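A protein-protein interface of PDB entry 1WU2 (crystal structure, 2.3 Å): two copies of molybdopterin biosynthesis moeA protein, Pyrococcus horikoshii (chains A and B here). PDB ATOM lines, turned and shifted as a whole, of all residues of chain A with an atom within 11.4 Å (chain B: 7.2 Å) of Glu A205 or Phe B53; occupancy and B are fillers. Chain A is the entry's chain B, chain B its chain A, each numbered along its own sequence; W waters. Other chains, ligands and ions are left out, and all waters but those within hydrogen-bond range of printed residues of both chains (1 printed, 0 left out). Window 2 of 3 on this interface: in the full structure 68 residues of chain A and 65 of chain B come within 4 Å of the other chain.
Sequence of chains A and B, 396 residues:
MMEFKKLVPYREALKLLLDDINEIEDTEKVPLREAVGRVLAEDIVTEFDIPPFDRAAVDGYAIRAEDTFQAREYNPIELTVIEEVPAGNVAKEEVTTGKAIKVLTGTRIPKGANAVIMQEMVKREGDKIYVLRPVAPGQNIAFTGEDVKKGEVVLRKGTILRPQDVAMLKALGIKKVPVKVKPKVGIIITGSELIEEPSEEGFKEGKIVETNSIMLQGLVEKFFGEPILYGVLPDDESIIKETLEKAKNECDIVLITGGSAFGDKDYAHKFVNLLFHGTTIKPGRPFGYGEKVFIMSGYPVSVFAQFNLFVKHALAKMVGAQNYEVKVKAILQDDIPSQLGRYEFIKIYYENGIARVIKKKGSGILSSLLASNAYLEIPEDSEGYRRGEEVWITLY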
ATOM      1  N   SER A 192     -31.063  29.260 -18.263  1.00  0.00           N
ATOM      2  CA  SER A 192     -29.805  29.949 -18.556  1.00  0.00           C
ATOM      3  C   SER A 192     -28.617  29.379 -17.774  1.00  0.00           C
ATOM      4  O   SER A 192     -27.465  29.581 -18.166  1.00  0.00           O
ATOM      5  CB  SER A 192     -29.943  31.450 -18.276  1.00  0.00           C
ATOM      6  OG  SER A 192     -30.343  31.688 -16.937  1.00  0.00           O
ATOM      7  N   GLU A 193     -28.890  28.661 -16.684  1.00  0.00           N
ATOM      8  CA  GLU A 193     -27.827  28.091 -15.852  1.00  0.00           C
ATOM      9  C   GLU A 193     -27.452  26.649 -16.220  1.00  0.00           C
ATOM     10  O   GLU A 193     -26.658  26.024 -15.522  1.00  0.00           O
ATOM     11  CB  GLU A 193     -28.216  28.164 -14.369  1.00  0.00           C
ATOM     12  CG  GLU A 193     -28.646  29.548 -13.884  1.00  0.00           C
ATOM     13  CD  GLU A 193     -27.720  30.666 -14.341  1.00  0.00           C
ATOM     14  OE1 GLU A 193     -26.482  30.477 -14.320  1.00  0.00           O
ATOM     15  OE2 GLU A 193     -28.232  31.741 -14.724  1.00  0.00           O
ATOM     16  N   LEU A 194     -27.993  26.133 -17.321  1.00  0.00           N
ATOM     17  CA  LEU A 194     -27.735  24.752 -17.726  1.00  0.00           C
ATOM     18  C   LEU A 194     -26.360  24.573 -18.369  1.00  0.00           C
ATOM     19  O   LEU A 194     -25.937  25.391 -19.184  1.00  0.00           O
ATOM     20  CB  LEU A 194     -28.811  24.273 -18.701  1.00  0.00           C
ATOM     21  CG  LEU A 194     -30.231  24.241 -18.139  1.00  0.00           C
ATOM     22  CD1 LEU A 194     -31.230  24.013 -19.255  1.00  0.00           C
ATOM     23  CD2 LEU A 194     -30.365  23.172 -17.064  1.00  0.00           C
ATOM     24  N   ILE A 195     -25.672  23.504 -17.974  1.00  0.00           N
ATOM     25  CA  ILE A 195     -24.474  23.022 -18.663  1.00  0.00           C
ATOM     26  C   ILE A 195     -24.678  21.556 -19.062  1.00  0.00           C
ATOM     27  O   ILE A 195     -25.658  20.931 -18.662  1.00  0.00           O
ATOM     28  CB  ILE A 195     -23.203  23.193 -17.787  1.00  0.00           C
ATOM     29  CG1 ILE A 195     -23.426  22.650 -16.372  1.00  0.00           C
ATOM     30  CG2 ILE A 195     -22.791  24.663 -17.742  1.00  0.00           C
ATOM     31  CD1 ILE A 195     -22.147  22.356 -15.628  1.00  0.00           C
ATOM     32  N   GLU A 197     -22.146  18.944 -18.908  1.00  0.00           N
ATOM     33  CA  GLU A 197     -21.372  17.961 -18.145  1.00  0.00           C
ATOM     34  C   GLU A 197     -20.661  18.577 -16.925  1.00  0.00           C
ATOM     35  O   GLU A 197     -20.331  19.761 -16.927  1.00  0.00           O
ATOM     36  CB  GLU A 197     -20.364  17.254 -19.066  1.00  0.00           C
ATOM     37  CG  GLU A 197     -19.331  18.164 -19.715  1.00  0.00           C
ATOM     38  CD  GLU A 197     -18.668  17.532 -20.931  1.00  0.00           C
ATOM     39  OE1 GLU A 197     -18.425  16.304 -20.918  1.00  0.00           O
ATOM     40  OE2 GLU A 197     -18.383  18.265 -21.905  1.00  0.00           O
ATOM     41  N   PRO A 198     -20.428  17.773 -15.888  1.00  0.00           N
ATOM     42  CA  PRO A 198     -19.861  18.277 -14.628  1.00  0.00           C
ATOM     43  C   PRO A 198     -18.401  18.733 -14.703  1.00  0.00           C
ATOM     44  O   PRO A 198     -17.980  19.495 -13.834  1.00  0.00           O
ATOM     45  CB  PRO A 198     -19.990  17.078 -13.683  1.00  0.00           C
ATOM     46  CG  PRO A 198     -19.979  15.901 -14.569  1.00  0.00           C
ATOM     47  CD  PRO A 198     -20.692  16.323 -15.818  1.00  0.00           C
ATOM     48  N   SER A 199     -17.653  18.284 -15.709  1.00  0.00           N
ATOM     49  CA  SER A 199     -16.250  18.670 -15.869  1.00  0.00           C
ATOM     50  C   SER A 199     -16.076  20.102 -16.389  1.00  0.00           C
ATOM     51  O   SER A 199     -14.983  20.664 -16.298  1.00  0.00           O
ATOM     52  CB  SER A 199     -15.529  17.693 -16.803  1.00  0.00           C
ATOM     53  OG  SER A 199     -16.005  17.811 -18.132  1.00  0.00           O
ATOM     54  N   GLU A 200     -17.138  20.680 -16.948  1.00  0.00           N
ATOM     55  CA  GLU A 200     -17.120  22.083 -17.375  1.00  0.00           C
ATOM     56  C   GLU A 200     -16.872  23.004 -16.184  1.00  0.00           C
ATOM     57  O   GLU A 200     -17.230  22.679 -15.048  1.00  0.00           O
ATOM     58  CB  GLU A 200     -18.439  22.473 -18.048  1.00  0.00           C
ATOM     59  CG  GLU A 200     -18.580  21.985 -19.478  1.00  0.00           C
ATOM     60  CD  GLU A 200     -19.877  22.441 -20.120  1.00  0.00           C
ATOM     61  OE1 GLU A 200     -20.167  23.657 -20.085  1.00  0.00           O
ATOM     62  OE2 GLU A 200     -20.610  21.583 -20.662  1.00  0.00           O
ATOM     63  N   GLU A 201     -16.261  24.153 -16.455  1.00  0.00           N
ATOM     64  CA  GLU A 201     -15.931  25.123 -15.410  1.00  0.00           C
ATOM     65  C   GLU A 201     -17.173  25.735 -14.750  1.00  0.00           C
ATOM     66  O   GLU A 201     -17.127  26.138 -13.587  1.00  0.00           O
ATOM     67  CB  GLU A 201     -15.002  26.222 -15.956  1.00  0.00           C
ATOM     68  CG  GLU A 201     -15.584  27.094 -17.068  1.00  0.00           C
ATOM     69  CD  GLU A 201     -14.535  27.978 -17.734  1.00  0.00           C
ATOM     70  OE1 GLU A 201     -14.833  28.560 -18.803  1.00  0.00           O
ATOM     71  OE2 GLU A 201     -13.413  28.098 -17.188  1.00  0.00           O
ATOM     72  N   GLY A 202     -18.283  25.786 -15.483  1.00  0.00           N
ATOM     73  CA  GLY A 202     -19.528  26.315 -14.954  1.00  0.00           C
ATOM     74  C   GLY A 202     -20.097  25.532 -13.778  1.00  0.00           C
ATOM     75  O   GLY A 202     -20.822  26.093 -12.961  1.00  0.00           O
ATOM     76  N   PHE A 203     -19.771  24.245 -13.695  1.00  0.00           N
ATOM     77  CA  PHE A 203     -20.303  23.364 -12.654  1.00  0.00           C
ATOM     78  C   PHE A 203     -19.946  23.814 -11.234  1.00  0.00           C
ATOM     79  O   PHE A 203     -20.789  23.774 -10.341  1.00  0.00           O
ATOM     80  CB  PHE A 203     -19.821  21.924 -12.873  1.00  0.00           C
ATOM     81  CG  PHE A 203     -20.323  20.958 -11.838  1.00  0.00           C
ATOM     82  CD1 PHE A 203     -19.455  20.399 -10.908  1.00  0.00           C
ATOM     83  CD2 PHE A 203     -21.666  20.618 -11.787  1.00  0.00           C
ATOM     84  CE1 PHE A 203     -19.920  19.512  -9.946  1.00  0.00           C
ATOM     85  CE2 PHE A 203     -22.137  19.733 -10.831  1.00  0.00           C
ATOM     86  CZ  PHE A 203     -21.261  19.180  -9.909  1.00  0.00           C
ATOM     87  N   LYS A 204     -18.699  24.234 -11.033  1.00  0.00           N
ATOM     88  CA  LYS A 204     -18.232  24.652  -9.710  1.00  0.00           C
ATOM     89  C   LYS A 204     -18.778  26.019  -9.286  1.00  0.00           C
ATOM     90  O   LYS A 204     -18.756  26.351  -8.102  1.00  0.00           O
ATOM     91  CB  LYS A 204     -16.701  24.640  -9.642  1.00  0.00           C
ATOM     92  CG  LYS A 204     -16.131  23.261  -9.315  1.00  0.00           C
ATOM     93  CD  LYS A 204     -14.672  23.111  -9.734  1.00  0.00           C
ATOM     94  CE  LYS A 204     -13.721  23.559  -8.633  1.00  0.00           C
ATOM     95  NZ  LYS A 204     -12.297  23.235  -8.937  1.00  0.00           N
ATOM     96  N   GLU A 205     -19.259  26.803 -10.251  1.00  0.00           N
ATOM     97  CA  GLU A 205     -19.892  28.091  -9.967  1.00  0.00           C
ATOM     98  C   GLU A 205     -21.392  27.955  -9.663  1.00  0.00           C
ATOM     99  O   GLU A 205     -22.011  28.897  -9.174  1.00  0.00           O
ATOM    100  CB  GLU A 205     -19.678  29.058 -11.138  1.00  0.00           C
ATOM    101  CG  GLU A 205     -18.228  29.493 -11.323  1.00  0.00           C
ATOM    102  CD  GLU A 205     -17.992  30.211 -12.641  1.00  0.00           C
ATOM    103  OE1 GLU A 205     -18.704  31.204 -12.918  1.00  0.00           O
ATOM    104  OE2 GLU A 205     -17.094  29.787 -13.405  1.00  0.00           O
ATOM    105  N   GLY A 206     -21.972  26.793  -9.958  1.00  0.00           N
ATOM    106  CA  GLY A 206     -23.375  26.530  -9.667  1.00  0.00           C
ATOM    107  C   GLY A 206     -24.249  26.194 -10.865  1.00  0.00           C
ATOM    108  O   GLY A 206     -25.456  26.017 -10.711  1.00  0.00           O
ATOM    109  N   LYS A 207     -23.664  26.117 -12.059  1.00  0.00           N
ATOM    110  CA  LYS A 207     -24.406  25.677 -13.241  1.00  0.00           C
ATOM    111  C   LYS A 207     -24.785  24.206 -13.076  1.00  0.00           C
ATOM    112  O   LYS A 207     -23.976  23.397 -12.619  1.00  0.00           O
ATOM    113  CB  LYS A 207     -23.586  25.864 -14.521  1.00  0.00           C
ATOM    114  CG  LYS A 207     -23.151  27.304 -14.810  1.00  0.00           C
ATOM    115  CD  LYS A 207     -24.107  28.012 -15.761  1.00  0.00           C
ATOM    116  CE  LYS A 207     -23.469  29.244 -16.397  1.00  0.00           C
ATOM    117  NZ  LYS A 207     -22.731  28.918 -17.658  1.00  0.00           N
ATOM    118  N   ILE A 208     -26.019  23.873 -13.445  1.00  0.00           N
ATOM    119  CA  ILE A 208     -26.588  22.546 -13.215  1.00  0.00           C
ATOM    120  C   ILE A 208     -26.504  21.687 -14.470  1.00  0.00           C
ATOM    121  O   ILE A 208     -26.870  22.135 -15.553  1.00  0.00           O
ATOM    122  CB  ILE A 208     -28.067  22.693 -12.785  1.00  0.00           C
ATOM    123  CG1 ILE A 208     -28.174  23.462 -11.458  1.00  0.00           C
ATOM    124  CG2 ILE A 208     -28.744  21.325 -12.674  1.00  0.00           C
ATOM    125  CD1 ILE A 208     -29.361  24.408 -11.398  1.00  0.00           C
ATOM    126  N   VAL A 209     -26.046  20.445 -14.319  1.00  0.00           N
ATOM    127  CA  VAL A 209     -26.012  19.506 -15.438  1.00  0.00           C
ATOM    128  C   VAL A 209     -27.445  19.186 -15.878  1.00  0.00           C
ATOM    129  O   VAL A 209     -28.315  18.914 -15.054  1.00  0.00           O
ATOM    130  CB  VAL A 209     -25.253  18.206 -15.090  1.00  0.00           C
ATOM    131  CG1 VAL A 209     -25.423  17.159 -16.190  1.00  0.00           C
ATOM    132  CG2 VAL A 209     -23.775  18.500 -14.866  1.00  0.00           C
ATOM    133  N   SER A 363     -33.270  20.590  -3.144  1.00  0.00           N
ATOM    134  CA  SER A 363     -33.426  21.685  -4.110  1.00  0.00           C
ATOM    135  C   SER A 363     -33.752  21.196  -5.526  1.00  0.00           C
ATOM    136  O   SER A 363     -34.588  21.788  -6.213  1.00  0.00           O
ATOM    137  CB  SER A 363     -32.167  22.562  -4.138  1.00  0.00           C
ATOM    138  OG  SER A 363     -32.169  23.492  -3.066  1.00  0.00           O
ATOM    139  N   GLY A 364     -33.086  20.128  -5.958  1.00  0.00           N
ATOM    140  CA  GLY A 364     -33.346  19.545  -7.266  1.00  0.00           C
ATOM    141  C   GLY A 364     -32.699  18.181  -7.415  1.00  0.00           C
ATOM    142  O   GLY A 364     -31.981  17.932  -8.385  1.00  0.00           O
ATOM    143  N   ILE A 365     -32.963  17.298  -6.454  1.00  0.00           N
ATOM    144  CA  ILE A 365     -32.262  16.014  -6.369  1.00  0.00           C
ATOM    145  C   ILE A 365     -32.799  14.954  -7.333  1.00  0.00           C
ATOM    146  O   ILE A 365     -33.952  15.005  -7.762  1.00  0.00           O
ATOM    147  CB  ILE A 365     -32.255  15.464  -4.914  1.00  0.00           C
ATOM    148  CG1 ILE A 365     -33.659  15.018  -4.479  1.00  0.00           C
ATOM    149  CG2 ILE A 365     -31.661  16.502  -3.960  1.00  0.00           C
ATOM    150  CD1 ILE A 365     -33.744  14.542  -3.036  1.00  0.00           C
ATOM    151  N   ASP B  49     -19.426  16.040  -6.171  1.00  0.00           N
ATOM    152  CA  ASP B  49     -20.493  16.386  -5.237  1.00  0.00           C
ATOM    153  C   ASP B  49     -21.604  17.108  -5.999  1.00  0.00           C
ATOM    154  O   ASP B  49     -21.327  18.002  -6.801  1.00  0.00           O
ATOM    155  CB  ASP B  49     -19.982  17.334  -4.140  1.00  0.00           C
ATOM    156  CG  ASP B  49     -18.994  16.683  -3.199  1.00  0.00           C
ATOM    157  OD1 ASP B  49     -19.402  15.807  -2.415  1.00  0.00           O
ATOM    158  OD2 ASP B  49     -17.793  17.009  -3.145  1.00  0.00           O
ATOM    159  N   ILE B  50     -22.850  16.721  -5.745  1.00  0.00           N
ATOM    160  CA  ILE B  50     -24.017  17.420  -6.279  1.00  0.00           C
ATOM    161  C   ILE B  50     -24.945  17.772  -5.109  1.00  0.00           C
ATOM    162  O   ILE B  50     -25.440  16.871  -4.437  1.00  0.00           O
ATOM    163  CB  ILE B  50     -24.768  16.552  -7.312  1.00  0.00           C
ATOM    164  CG1 ILE B  50     -23.855  16.213  -8.496  1.00  0.00           C
ATOM    165  CG2 ILE B  50     -26.033  17.285  -7.811  1.00  0.00           C
ATOM    166  CD1 ILE B  50     -24.396  15.132  -9.409  1.00  0.00           C
ATOM    167  N   PRO B  51     -25.160  19.060  -4.830  1.00  0.00           N
ATOM    168  CA  PRO B  51     -24.475  20.172  -5.502  1.00  0.00           C
ATOM    169  C   PRO B  51     -23.009  20.237  -5.071  1.00  0.00           C
ATOM    170  O   PRO B  51     -22.669  19.660  -4.039  1.00  0.00           O
ATOM    171  CB  PRO B  51     -25.241  21.400  -5.002  1.00  0.00           C
ATOM    172  CG  PRO B  51     -25.768  20.993  -3.673  1.00  0.00           C
ATOM    173  CD  PRO B  51     -26.096  19.532  -3.797  1.00  0.00           C
ATOM    174  N   PRO B  52     -22.155  20.916  -5.831  1.00  0.00           N
ATOM    175  CA  PRO B  52     -20.721  20.950  -5.511  1.00  0.00           C
ATOM    176  C   PRO B  52     -20.354  21.809  -4.290  1.00  0.00           C
ATOM    177  O   PRO B  52     -19.240  21.662  -3.781  1.00  0.00           O
ATOM    178  CB  PRO B  52     -20.082  21.495  -6.794  1.00  0.00           C
ATOM    179  CG  PRO B  52     -21.158  22.236  -7.499  1.00  0.00           C
ATOM    180  CD  PRO B  52     -22.479  21.696  -7.035  1.00  0.00           C
ATOM    181  N   PHE B  53     -21.256  22.684  -3.837  1.00  0.00           N
ATOM    182  CA  PHE B  53     -21.015  23.501  -2.640  1.00  0.00           C
ATOM    183  C   PHE B  53     -22.288  23.757  -1.821  1.00  0.00           C
ATOM    184  O   PHE B  53     -23.395  23.458  -2.265  1.00  0.00           O
ATOM    185  CB  PHE B  53     -20.334  24.831  -3.007  1.00  0.00           C
ATOM    186  CG  PHE B  53     -21.047  25.613  -4.076  1.00  0.00           C
ATOM    187  CD1 PHE B  53     -21.985  26.573  -3.738  1.00  0.00           C
ATOM    188  CD2 PHE B  53     -20.769  25.400  -5.416  1.00  0.00           C
ATOM    189  CE1 PHE B  53     -22.641  27.309  -4.718  1.00  0.00           C
ATOM    190  CE2 PHE B  53     -21.425  26.131  -6.405  1.00  0.00           C
ATOM    191  CZ  PHE B  53     -22.363  27.083  -6.052  1.00  0.00           C
ATOM    192  N   ASP B  54     -22.109  24.291  -0.612  1.00  0.00           N
ATOM    193  CA  ASP B  54     -23.230  24.662   0.257  1.00  0.00           C
ATOM    194  C   ASP B  54     -23.965  25.840  -0.374  1.00  0.00           C
ATOM    195  O   ASP B  54     -23.352  26.860  -0.661  1.00  0.00           O
ATOM    196  CB  ASP B  54     -22.749  25.073   1.660  1.00  0.00           C
ATOM    197  CG  ASP B  54     -21.957  23.982   2.370  1.00  0.00           C
ATOM    198  OD1 ASP B  54     -22.127  22.792   2.045  1.00  0.00           O
ATOM    199  OD2 ASP B  54     -21.137  24.229   3.281  1.00  0.00           O
ATOM    200  N   ARG B  55     -25.274  25.696  -0.575  1.00  0.00           N
ATOM    201  CA  ARG B  55     -26.091  26.708  -1.243  1.00  0.00           C
ATOM    202  C   ARG B  55     -27.197  27.218  -0.337  1.00  0.00           C
ATOM    203  O   ARG B  55     -27.695  26.491   0.516  1.00  0.00           O
ATOM    204  CB  ARG B  55     -26.754  26.116  -2.485  1.00  0.00           C
ATOM    205  CG  ARG B  55     -25.797  25.532  -3.511  1.00  0.00           C
ATOM    206  CD  ARG B  55     -25.920  26.166  -4.884  1.00  0.00           C
ATOM    207  NE  ARG B  55     -25.865  25.197  -5.966  1.00  0.00           N
ATOM    208  CZ  ARG B  55     -25.973  25.507  -7.253  1.00  0.00           C
ATOM    209  NH1 ARG B  55     -26.145  26.773  -7.633  1.00  0.00           N
ATOM    210  NH2 ARG B  55     -25.905  24.542  -8.164  1.00  0.00           N
ATOM    211  N   ALA B  56     -27.599  28.466  -0.544  1.00  0.00           N
ATOM    212  CA  ALA B  56     -28.804  28.987   0.082  1.00  0.00           C
ATOM    213  C   ALA B  56     -30.002  28.383  -0.650  1.00  0.00           C
ATOM    214  O   ALA B  56     -30.078  28.451  -1.870  1.00  0.00           O
ATOM    215  CB  ALA B  56     -28.832  30.500  -0.005  1.00  0.00           C
ATOM    216  N   GLY B  88     -25.591  35.449  -8.870  1.00  0.00           N
ATOM    217  CA  GLY B  88     -24.491  34.678  -9.430  1.00  0.00           C
ATOM    218  C   GLY B  88     -23.101  35.058  -8.934  1.00  0.00           C
ATOM    219  O   GLY B  88     -22.102  34.676  -9.546  1.00  0.00           O
ATOM    220  N   ASN B  89     -23.035  35.796  -7.828  1.00  0.00           N
ATOM    221  CA  ASN B  89     -21.768  36.241  -7.251  1.00  0.00           C
ATOM    222  C   ASN B  89     -21.459  35.454  -5.980  1.00  0.00           C
ATOM    223  O   ASN B  89     -22.258  34.624  -5.545  1.00  0.00           O
ATOM    224  CB  ASN B  89     -21.819  37.747  -6.938  1.00  0.00           C
ATOM    225  CG  ASN B  89     -21.296  38.609  -8.079  1.00  0.00           C
ATOM    226  OD1 ASN B  89     -20.627  39.619  -7.850  1.00  0.00           O
ATOM    227  ND2 ASN B  89     -21.604  38.218  -9.311  1.00  0.00           N
ATOM    228  N   VAL B  90     -20.288  35.720  -5.404  1.00  0.00           N
ATOM    229  CA  VAL B  90     -19.882  35.159  -4.118  1.00  0.00           C
ATOM    230  C   VAL B  90     -19.639  36.300  -3.127  1.00  0.00           C
ATOM    231  O   VAL B  90     -19.230  37.394  -3.518  1.00  0.00           O
ATOM    232  CB  VAL B  90     -18.596  34.308  -4.260  1.00  0.00           C
ATOM    233  CG1 VAL B  90     -18.181  33.709  -2.920  1.00  0.00           C
ATOM    234  CG2 VAL B  90     -18.793  33.207  -5.294  1.00  0.00           C
ATOM    235  N   GLY B 106     -29.300  29.693  -4.428  1.00  0.00           N
ATOM    236  CA  GLY B 106     -28.196  29.252  -5.262  1.00  0.00           C
ATOM    237  C   GLY B 106     -26.845  29.801  -4.826  1.00  0.00           C
ATOM    238  O   GLY B 106     -25.809  29.211  -5.125  1.00  0.00           O
ATOM    239  N   THR B 107     -26.851  30.930  -4.119  1.00  0.00           N
ATOM    240  CA  THR B 107     -25.612  31.589  -3.706  1.00  0.00           C
ATOM    241  C   THR B 107     -24.861  30.746  -2.678  1.00  0.00           C
ATOM    242  O   THR B 107     -25.464  30.183  -1.768  1.00  0.00           O
ATOM    243  CB  THR B 107     -25.910  32.977  -3.106  1.00  0.00           C
ATOM    244  OG1 THR B 107     -26.722  33.738  -4.006  1.00  0.00           O
ATOM    245  CG2 THR B 107     -24.638  33.806  -2.972  1.00  0.00           C
ATOM    246  N   ARG B 108     -23.543  30.676  -2.829  1.00  0.00           N
ATOM    247  CA  ARG B 108     -22.700  29.934  -1.905  1.00  0.00           C
ATOM    248  C   ARG B 108     -22.765  30.577  -0.528  1.00  0.00           C
ATOM    249  O   ARG B 108     -22.662  31.794  -0.407  1.00  0.00           O
ATOM    250  CB  ARG B 108     -21.254  29.912  -2.399  1.00  0.00           C
ATOM    251  CG  ARG B 108     -20.346  28.982  -1.610  1.00  0.00           C
ATOM    252  CD  ARG B 108     -18.907  29.434  -1.579  1.00  0.00           C
ATOM    253  NE  ARG B 108     -18.224  29.120  -2.829  1.00  0.00           N
ATOM    254  CZ  ARG B 108     -17.156  29.756  -3.302  1.00  0.00           C
ATOM    255  NH1 ARG B 108     -16.604  30.765  -2.635  1.00  0.00           N
ATOM    256  NH2 ARG B 108     -16.631  29.365  -4.457  1.00  0.00           N
ATOM    257  N   ILE B 109     -22.945  29.758   0.502  1.00  0.00           N
ATOM    258  CA  ILE B 109     -23.014  30.258   1.868  1.00  0.00           C
ATOM    259  C   ILE B 109     -21.674  30.913   2.195  1.00  0.00           C
ATOM    260  O   ILE B 109     -20.629  30.274   2.068  1.00  0.00           O
ATOM    261  CB  ILE B 109     -23.326  29.117   2.873  1.00  0.00           C
ATOM    262  CG1 ILE B 109     -24.665  28.435   2.548  1.00  0.00           C
ATOM    263  CG2 ILE B 109     -23.344  29.648   4.300  1.00  0.00           C
ATOM    264  CD1 ILE B 109     -25.840  29.374   2.380  1.00  0.00           C
ATOM    265  N   ILE B 141     -30.104  25.429   4.021  1.00  0.00           N
ATOM    266  CA  ILE B 141     -28.860  25.178   3.306  1.00  0.00           C
ATOM    267  C   ILE B 141     -28.928  23.826   2.603  1.00  0.00           C
ATOM    268  O   ILE B 141     -29.077  22.788   3.249  1.00  0.00           O
ATOM    269  CB  ILE B 141     -27.642  25.228   4.252  1.00  0.00           C
ATOM    270  CG1 ILE B 141     -27.416  26.660   4.738  1.00  0.00           C
ATOM    271  CG2 ILE B 141     -26.388  24.718   3.533  1.00  0.00           C
ATOM    272  CD1 ILE B 141     -26.356  26.799   5.810  1.00  0.00           C
ATOM    273  N   ALA B 142     -28.840  23.859   1.278  1.00  0.00           N
ATOM    274  CA  ALA B 142     -28.569  22.667   0.489  1.00  0.00           C
ATOM    275  C   ALA B 142     -27.077  22.358   0.590  1.00  0.00           C
ATOM    276  O   ALA B 142     -26.264  22.914  -0.148  1.00  0.00           O
ATOM    277  CB  ALA B 142     -28.982  22.879  -0.964  1.00  0.00           C
ATOM    278  N   PHE B 143     -26.722  21.473   1.514  1.00  0.00           N
ATOM    279  CA  PHE B 143     -25.319  21.148   1.773  1.00  0.00           C
ATOM    280  C   PHE B 143     -24.663  20.420   0.604  1.00  0.00           C
ATOM    281  O   PHE B 143     -25.337  19.877  -0.269  1.00  0.00           O
ATOM    282  CB  PHE B 143     -25.191  20.301   3.045  1.00  0.00           C
ATOM    283  CG  PHE B 143     -25.320  21.094   4.312  1.00  0.00           C
ATOM    284  CD1 PHE B 143     -24.272  21.887   4.755  1.00  0.00           C
ATOM    285  CD2 PHE B 143     -26.489  21.049   5.062  1.00  0.00           C
ATOM    286  CE1 PHE B 143     -24.383  22.622   5.931  1.00  0.00           C
ATOM    287  CE2 PHE B 143     -26.609  21.781   6.236  1.00  0.00           C
ATOM    288  CZ  PHE B 143     -25.553  22.569   6.670  1.00  0.00           C
ATOM    289  N   THR B 144     -23.334  20.410   0.613  1.00  0.00           N
ATOM    290  CA  THR B 144     -22.543  19.774  -0.430  1.00  0.00           C
ATOM    291  C   THR B 144     -22.842  18.281  -0.483  1.00  0.00           C
ATOM    292  O   THR B 144     -22.684  17.572   0.510  1.00  0.00           O
ATOM    293  CB  THR B 144     -21.037  20.003  -0.168  1.00  0.00           C
ATOM    294  OG1 THR B 144     -20.734  21.399  -0.273  1.00  0.00           O
ATOM    295  CG2 THR B 144     -20.171  19.356  -1.250  1.00  0.00           C
ATOM    296  N   GLY B 145     -23.299  17.821  -1.643  1.00  0.00           N
ATOM    297  CA  GLY B 145     -23.498  16.407  -1.884  1.00  0.00           C
ATOM    298  C   GLY B 145     -24.770  15.834  -1.291  1.00  0.00           C
ATOM    299  O   GLY B 145     -24.876  14.620  -1.131  1.00  0.00           O
HETATM  300  O   HOH W   1     -27.432  27.852 -10.612  1.00  0.00           O
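Along chain B the printed residues that touch a printed residue of chain A span positions 49 to 142. Among the printed residues, 7 pairs touch across the chains. Among the printed residues, no Asp or Glu carboxylate lies within 4 Å of a Lys or Arg side-chain nitrogen of the other chain.
Of chain B, only Phe B53 (3.6 Å) comes within 4 Å of Glu A205. Phe B53 touches just these residues of chain A: Lys A204, Glu A205 and Gly A206. Asp B49 touches just one residue of chain A: Phe A203. No residue of chain A comes within 4 Å of Pro B51. Pro B52 touches one residue of chain A. No residue of chain A comes within 4 Å of Asp B54. Printed residues of chain A within 4 Å of Arg B55: Gly A206 (3.0 Å). No residue of chain A comes within 4 Å of Gly B106. No residue of chain A comes within 4 Å of Arg B108. Printed residues of chain B within 4 Å of Gly A206: Phe B53 (3.7 Å) and Arg B55 (3.0 Å). Of the printed residues of chain B, Phe A203 touches Asp B49 and Pro B52. Printed residues of chain B within 4 Å of Lys A204: Phe B53. Printed residues of chain B within 4 Å of Ser A363: Ala B142. Lys A207 touches none of the printed residues of chain B. The nearest residue of chain A that does not touch Phe B53 is Phe A203 (4.6 Å).
The backbone NH of Ala B142 lies within hydrogen-bond range of the backbone carbonyl oxygen of Arg B55, at 3.0 Å.
Among the printed residues, pairs that only touch across the chains: Phe A203 with Asp B49, Phe A203 with Pro B52, Lys A204 with Phe B53, Glu A205 with Phe B53, Gly A206 with Phe B53 and Ser A363 with Ala B142.
No position is printed for both chains.
Water W1 bridges the backbone carbonyl oxygen (O) of Gly A206 (2.7 Å) and the guanidinium group (NH1) of Arg B55 (3.4 Å).
NH2 of Arg B55 sits at hydrogen-bond distance from O of Gly A206, 3.0 Å away.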
